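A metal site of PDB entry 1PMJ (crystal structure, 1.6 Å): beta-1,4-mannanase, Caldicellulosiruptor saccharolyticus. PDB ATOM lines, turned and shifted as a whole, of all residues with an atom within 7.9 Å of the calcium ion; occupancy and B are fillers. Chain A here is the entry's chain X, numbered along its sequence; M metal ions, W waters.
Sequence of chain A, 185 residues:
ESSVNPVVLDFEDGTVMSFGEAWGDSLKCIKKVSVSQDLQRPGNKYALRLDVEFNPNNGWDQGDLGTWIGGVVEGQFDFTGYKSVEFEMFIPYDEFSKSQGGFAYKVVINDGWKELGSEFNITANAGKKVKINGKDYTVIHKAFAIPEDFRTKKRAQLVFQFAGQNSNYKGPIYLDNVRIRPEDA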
ATOM      1  N   LEU A   9     -29.865  15.276  31.469  1.00  0.00           N
ATOM      2  CA  LEU A   9     -30.441  16.353  30.643  1.00  0.00           C
ATOM      3  C   LEU A   9     -29.497  17.548  30.752  1.00  0.00           C
ATOM      4  O   LEU A   9     -29.641  18.447  31.596  1.00  0.00           O
ATOM      5  CB  LEU A   9     -31.894  16.690  31.074  1.00  0.00           C
ATOM      6  CG  LEU A   9     -32.786  15.465  31.297  1.00  0.00           C
ATOM      7  CD1 LEU A   9     -34.158  15.893  31.768  1.00  0.00           C
ATOM      8  CD2 LEU A   9     -32.867  14.676  30.040  1.00  0.00           C
ATOM      9  N   ASP A  10     -28.499  17.501  29.900  1.00  0.00           N
ATOM     10  CA  ASP A  10     -27.409  18.475  29.838  1.00  0.00           C
ATOM     11  C   ASP A  10     -27.466  19.396  28.602  1.00  0.00           C
ATOM     12  O   ASP A  10     -26.555  20.200  28.391  1.00  0.00           O
ATOM     13  CB  ASP A  10     -26.051  17.773  29.944  1.00  0.00           C
ATOM     14  CG  ASP A  10     -25.769  16.797  28.791  1.00  0.00           C
ATOM     15  OD1 ASP A  10     -26.564  16.722  27.815  1.00  0.00           O
ATOM     16  OD2 ASP A  10     -24.730  16.071  28.788  1.00  0.00           O
ATOM     17  N   PHE A  11     -28.469  19.218  27.764  1.00  0.00           N
ATOM     18  CA  PHE A  11     -28.716  20.046  26.564  1.00  0.00           C
ATOM     19  C   PHE A  11     -27.613  19.911  25.529  1.00  0.00           C
ATOM     20  O   PHE A  11     -27.569  20.678  24.582  1.00  0.00           O
ATOM     21  CB  PHE A  11     -29.009  21.514  26.980  1.00  0.00           C
ATOM     22  CG  PHE A  11     -30.050  21.567  28.056  1.00  0.00           C
ATOM     23  CD1 PHE A  11     -31.390  21.371  27.724  1.00  0.00           C
ATOM     24  CD2 PHE A  11     -29.695  21.721  29.414  1.00  0.00           C
ATOM     25  CE1 PHE A  11     -32.371  21.305  28.676  1.00  0.00           C
ATOM     26  CE2 PHE A  11     -30.675  21.647  30.377  1.00  0.00           C
ATOM     27  CZ  PHE A  11     -32.007  21.456  30.031  1.00  0.00           C
ATOM     28  N   GLU A  12     -26.731  18.915  25.674  1.00  0.00           N
ATOM     29  CA  GLU A  12     -25.539  18.863  24.825  1.00  0.00           C
ATOM     30  C   GLU A  12     -25.826  18.387  23.392  1.00  0.00           C
ATOM     31  O   GLU A  12     -24.972  18.497  22.517  1.00  0.00           O
ATOM     32  CB  GLU A  12     -24.428  18.052  25.470  1.00  0.00           C
ATOM     33  CG  GLU A  12     -23.843  18.712  26.698  1.00  0.00           C
ATOM     34  CD  GLU A  12     -23.329  20.112  26.407  1.00  0.00           C
ATOM     35  OE1 GLU A  12     -22.400  20.276  25.588  1.00  0.00           O
ATOM     36  OE2 GLU A  12     -23.885  21.069  26.995  1.00  0.00           O
ATOM     37  N   ASP A  13     -27.038  17.905  23.162  1.00  0.00           N
ATOM     38  CA  ASP A  13     -27.519  17.664  21.789  1.00  0.00           C
ATOM     39  C   ASP A  13     -28.048  18.890  21.050  1.00  0.00           C
ATOM     40  O   ASP A  13     -28.523  18.808  19.880  1.00  0.00           O
ATOM     41  CB  ASP A  13     -28.490  16.494  21.790  1.00  0.00           C
ATOM     42  CG  ASP A  13     -29.838  16.795  22.402  1.00  0.00           C
ATOM     43  OD1 ASP A  13     -30.053  17.899  22.933  1.00  0.00           O
ATOM     44  OD2 ASP A  13     -30.772  15.924  22.375  1.00  0.00           O
ATOM     45  N   MET A  17     -34.510  19.445  25.079  1.00  0.00           N
ATOM     46  CA  MET A  17     -34.744  18.187  25.753  1.00  0.00           C
ATOM     47  C   MET A  17     -36.112  18.120  26.447  1.00  0.00           C
ATOM     48  O   MET A  17     -36.236  17.768  27.633  1.00  0.00           O
ATOM     49  CB  MET A  17     -33.582  17.866  26.715  1.00  0.00           C
ATOM     50  CG  MET A  17     -32.256  17.618  26.010  1.00  0.00           C
ATOM     51  SD  MET A  17     -30.993  17.046  27.175  1.00  0.00           S
ATOM     52  CE  MET A  17     -29.716  16.374  26.052  1.00  0.00           C
ATOM     53  N   VAL A  35     -32.712  26.896  23.990  1.00  0.00           N
ATOM     54  CA  VAL A  35     -31.412  26.288  24.137  1.00  0.00           C
ATOM     55  C   VAL A  35     -30.384  27.324  23.678  1.00  0.00           C
ATOM     56  O   VAL A  35     -30.579  28.003  22.665  1.00  0.00           O
ATOM     57  CB  VAL A  35     -31.294  24.898  23.442  1.00  0.00           C
ATOM     58  CG1 VAL A  35     -31.597  24.956  21.932  1.00  0.00           C
ATOM     59  CG2 VAL A  35     -29.931  24.286  23.780  1.00  0.00           C
ATOM     60  N   SER A  36     -29.329  27.493  24.480  1.00  0.00           N
ATOM     61  CA  SER A  36     -28.423  28.633  24.396  1.00  0.00           C
ATOM     62  C   SER A  36     -26.983  28.231  24.481  1.00  0.00           C
ATOM     63  O   SER A  36     -26.637  27.286  25.197  1.00  0.00           O
ATOM     64  CB  SER A  36     -28.694  29.625  25.534  1.00  0.00           C
ATOM     65  OG  SER A  36     -27.884  30.791  25.467  1.00  0.00           O
ATOM     66  N   LEU A  39     -23.244  30.175  27.573  1.00  0.00           N
ATOM     67  CA  LEU A  39     -22.264  29.630  28.549  1.00  0.00           C
ATOM     68  C   LEU A  39     -21.303  28.627  27.913  1.00  0.00           C
ATOM     69  O   LEU A  39     -20.580  27.920  28.606  1.00  0.00           O
ATOM     70  CB  LEU A  39     -22.989  29.012  29.758  1.00  0.00           C
ATOM     71  CG  LEU A  39     -24.099  29.883  30.389  1.00  0.00           C
ATOM     72  CD1 LEU A  39     -24.720  29.160  31.617  1.00  0.00           C
ATOM     73  CD2 LEU A  39     -23.604  31.250  30.791  1.00  0.00           C
ATOM     74  N   ARG A  41     -18.451  26.602  26.701  1.00  0.00           N
ATOM     75  CA  ARG A  41     -17.107  26.522  27.258  1.00  0.00           C
ATOM     76  C   ARG A  41     -16.623  25.083  27.105  1.00  0.00           C
ATOM     77  O   ARG A  41     -17.426  24.207  26.743  1.00  0.00           O
ATOM     78  CB  ARG A  41     -17.109  26.980  28.719  1.00  0.00           C
ATOM     79  CG  ARG A  41     -17.992  26.157  29.659  1.00  0.00           C
ATOM     80  CD  ARG A  41     -18.303  26.930  30.924  1.00  0.00           C
ATOM     81  NE  ARG A  41     -19.020  26.194  31.942  1.00  0.00           N
ATOM     82  CZ  ARG A  41     -20.326  25.979  31.979  1.00  0.00           C
ATOM     83  NH1 ARG A  41     -21.106  26.424  31.013  1.00  0.00           N
ATOM     84  NH2 ARG A  41     -20.850  25.339  33.043  1.00  0.00           N
ATOM     85  N   GLY A  43     -16.133  21.414  27.234  1.00  0.00           N
ATOM     86  CA  GLY A  43     -16.921  20.355  27.841  1.00  0.00           C
ATOM     87  C   GLY A  43     -18.399  20.616  28.034  1.00  0.00           C
ATOM     88  O   GLY A  43     -19.137  19.746  28.545  1.00  0.00           O
ATOM     89  N   ASN A  44     -18.859  21.802  27.656  1.00  0.00           N
ATOM     90  CA  ASN A  44     -20.228  22.195  27.982  1.00  0.00           C
ATOM     91  C   ASN A  44     -20.687  23.329  27.051  1.00  0.00           C
ATOM     92  O   ASN A  44     -20.494  24.511  27.343  1.00  0.00           O
ATOM     93  CB  ASN A  44     -20.349  22.619  29.441  1.00  0.00           C
ATOM     94  CG  ASN A  44     -21.794  22.762  29.909  1.00  0.00           C
ATOM     95  OD1 ASN A  44     -22.724  22.843  29.097  1.00  0.00           O
ATOM     96  ND2 ASN A  44     -21.994  22.805  31.218  1.00  0.00           N
ATOM     97  N   LYS A  45     -21.326  22.913  25.953  1.00  0.00           N
ATOM     98  CA  LYS A  45     -21.684  23.854  24.893  1.00  0.00           C
ATOM     99  C   LYS A  45     -23.012  24.566  25.071  1.00  0.00           C
ATOM    100  O   LYS A  45     -23.134  25.717  24.665  1.00  0.00           O
ATOM    101  CB  LYS A  45     -21.696  23.118  23.557  1.00  0.00           C
ATOM    102  CG  LYS A  45     -21.943  24.028  22.350  1.00  0.00           C
ATOM    103  CD  LYS A  45     -21.524  23.351  21.064  1.00  0.00           C
ATOM    104  CE  LYS A  45     -21.817  24.233  19.874  1.00  0.00           C
ATOM    105  NZ  LYS A  45     -21.174  23.718  18.639  1.00  0.00           N
ATOM    106  N   TYR A  46     -24.017  23.885  25.626  1.00  0.00           N
ATOM    107  CA  TYR A  46     -25.372  24.391  25.654  1.00  0.00           C
ATOM    108  C   TYR A  46     -25.937  24.374  27.071  1.00  0.00           C
ATOM    109  O   TYR A  46     -25.575  23.551  27.909  1.00  0.00           O
ATOM    110  CB  TYR A  46     -26.290  23.549  24.777  1.00  0.00           C
ATOM    111  CG  TYR A  46     -25.916  23.429  23.326  1.00  0.00           C
ATOM    112  CD1 TYR A  46     -26.282  24.401  22.434  1.00  0.00           C
ATOM    113  CD2 TYR A  46     -25.260  22.308  22.838  1.00  0.00           C
ATOM    114  CE1 TYR A  46     -25.972  24.293  21.086  1.00  0.00           C
ATOM    115  CE2 TYR A  46     -24.931  22.186  21.496  1.00  0.00           C
ATOM    116  CZ  TYR A  46     -25.318  23.186  20.619  1.00  0.00           C
ATOM    117  OH  TYR A  46     -25.026  23.079  19.245  1.00  0.00           O
ATOM    118  N   ALA A  47     -26.877  25.283  27.310  1.00  0.00           N
ATOM    119  CA  ALA A  47     -27.676  25.304  28.545  1.00  0.00           C
ATOM    120  C   ALA A  47     -29.076  25.784  28.178  1.00  0.00           C
ATOM    121  O   ALA A  47     -29.318  26.314  27.079  1.00  0.00           O
ATOM    122  CB  ALA A  47     -26.999  26.216  29.605  1.00  0.00           C
ATOM    123  N   LEU A  48     -30.011  25.585  29.087  1.00  0.00           N
ATOM    124  CA  LEU A  48     -31.378  26.031  28.871  1.00  0.00           C
ATOM    125  C   LEU A  48     -31.532  27.427  29.429  1.00  0.00           C
ATOM    126  O   LEU A  48     -31.361  27.656  30.595  1.00  0.00           O
ATOM    127  CB  LEU A  48     -32.332  25.058  29.564  1.00  0.00           C
ATOM    128  CG  LEU A  48     -33.798  25.232  29.204  1.00  0.00           C
ATOM    129  CD1 LEU A  48     -34.074  24.687  27.806  1.00  0.00           C
ATOM    130  CD2 LEU A  48     -34.708  24.538  30.183  1.00  0.00           C
ATOM    131  N   GLU A  88     -28.008  22.330  38.127  1.00  0.00           N
ATOM    132  CA  GLU A  88     -27.341  23.607  38.315  1.00  0.00           C
ATOM    133  C   GLU A  88     -28.133  24.741  37.698  1.00  0.00           C
ATOM    134  O   GLU A  88     -28.734  24.571  36.628  1.00  0.00           O
ATOM    135  CB  GLU A  88     -25.970  23.576  37.660  1.00  0.00           C
ATOM    136  CG  GLU A  88     -24.998  22.593  38.260  1.00  0.00           C
ATOM    137  CD  GLU A  88     -23.629  22.680  37.626  1.00  0.00           C
ATOM    138  OE1 GLU A  88     -23.523  22.471  36.424  1.00  0.00           O
ATOM    139  OE2 GLU A  88     -22.680  23.075  38.314  1.00  0.00           O
ATOM    140  N   PHE A  90     -27.682  29.054  36.828  1.00  0.00           N
ATOM    141  CA  PHE A  90     -26.730  30.138  36.661  1.00  0.00           C
ATOM    142  C   PHE A  90     -27.509  31.435  36.414  1.00  0.00           C
ATOM    143  O   PHE A  90     -28.391  31.483  35.538  1.00  0.00           O
ATOM    144  CB  PHE A  90     -25.807  29.909  35.428  1.00  0.00           C
ATOM    145  CG  PHE A  90     -25.066  28.592  35.447  1.00  0.00           C
ATOM    146  CD1 PHE A  90     -25.748  27.402  35.193  1.00  0.00           C
ATOM    147  CD2 PHE A  90     -23.726  28.540  35.730  1.00  0.00           C
ATOM    148  CE1 PHE A  90     -25.075  26.152  35.206  1.00  0.00           C
ATOM    149  CE2 PHE A  90     -23.065  27.331  35.774  1.00  0.00           C
ATOM    150  CZ  PHE A  90     -23.753  26.138  35.500  1.00  0.00           C
ATOM    151  N   LEU A 175     -30.486  26.878  33.235  1.00  0.00           N
ATOM    152  CA  LEU A 175     -30.544  25.577  33.848  1.00  0.00           C
ATOM    153  C   LEU A 175     -29.632  24.633  33.054  1.00  0.00           C
ATOM    154  O   LEU A 175     -29.601  24.667  31.832  1.00  0.00           O
ATOM    155  CB  LEU A 175     -31.974  25.061  33.836  1.00  0.00           C
ATOM    156  CG  LEU A 175     -32.366  23.779  34.509  1.00  0.00           C
ATOM    157  CD1 LEU A 175     -32.150  23.932  36.026  1.00  0.00           C
ATOM    158  CD2 LEU A 175     -33.784  23.439  34.204  1.00  0.00           C
ATOM    159  N   ASP A 176     -28.886  23.807  33.761  1.00  0.00           N
ATOM    160  CA  ASP A 176     -28.017  22.835  33.109  1.00  0.00           C
ATOM    161  C   ASP A 176     -27.801  21.626  33.986  1.00  0.00           C
ATOM    162  O   ASP A 176     -28.074  21.637  35.184  1.00  0.00           O
ATOM    163  CB  ASP A 176     -26.663  23.485  32.753  1.00  0.00           C
ATOM    164  CG  ASP A 176     -25.960  22.855  31.542  1.00  0.00           C
ATOM    165  OD1 ASP A 176     -26.476  21.841  30.967  1.00  0.00           O
ATOM    166  OD2 ASP A 176     -24.887  23.339  31.090  1.00  0.00           O
ATOM    167  N   ASN A 177     -27.304  20.565  33.373  1.00  0.00           N
ATOM    168  CA  ASN A 177     -26.871  19.369  34.087  1.00  0.00           C
ATOM    169  C   ASN A 177     -27.926  18.845  35.063  1.00  0.00           C
ATOM    170  O   ASN A 177     -27.654  18.538  36.227  1.00  0.00           O
ATOM    171  CB  ASN A 177     -25.557  19.693  34.762  1.00  0.00           C
ATOM    172  CG  ASN A 177     -24.432  19.860  33.755  1.00  0.00           C
ATOM    173  OD1 ASN A 177     -24.479  19.271  32.679  1.00  0.00           O
ATOM    174  ND2 ASN A 177     -23.420  20.643  34.114  1.00  0.00           N
ATOM    175  N   VAL A 178     -29.133  18.689  34.549  1.00  0.00           N
ATOM    176  CA  VAL A 178     -30.217  18.070  35.291  1.00  0.00           C
ATOM    177  C   VAL A 178     -30.047  16.566  35.168  1.00  0.00           C
ATOM    178  O   VAL A 178     -30.099  16.025  34.058  1.00  0.00           O
ATOM    179  CB  VAL A 178     -31.593  18.513  34.741  1.00  0.00           C
ATOM    180  CG1 VAL A 178     -32.726  17.811  35.475  1.00  0.00           C
ATOM    181  CG2 VAL A 178     -31.756  20.031  34.839  1.00  0.00           C
HETATM  182 CA    CA M   1     -24.839  21.741  29.069  1.00  0.00          CA
HETATM  183  O   HOH W   1     -23.627  20.118  30.306  1.00  0.00           O
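Water W1 lies within hydrogen-bond range of the side-chain amide oxygen of Asn 177 and the side-chain amide nitrogen of Asn 44.
O of Tyr 46 is bound to the calcium ion, 2.3 Å away. Water W1 binds the calcium ion (2.4 Å). OE2 of Glu 12 is bound to the calcium ion. OD1 of Asn 44 binds the calcium ion, 2.4 Å away. The calcium ion is bound by the backbone carbonyl oxygen (O) of Asp 10 (2.4 Å). The calcium ion is bound by OD1 of Asp 176 (2.5 Å). OD2 of Asp 176 is bound to the calcium ion (2.6 Å).
The side-chain carboxylate (OE1) of Glu 12 lies within hydrogen-bond range of the backbone NH (N) of Lys 45 (2.9 Å). The guanidinium group (NH2) of Arg 41 sits close to the side-chain amide nitrogen (ND2) of Asn 44 (3.3 Å). SD of Met 17 lies within hydrogen-bond range of N of Asp 10. The backbone NH (N) of Asp 176 is in hydrogen-bond range of the backbone carbonyl oxygen (O) of Glu 88, 3.0 Å away.
Of the 22 residues printed, 5 come within 4 Å of the calcium ion. Along chain A the residues within 4 Å of the calcium ion span positions 10 to 176.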
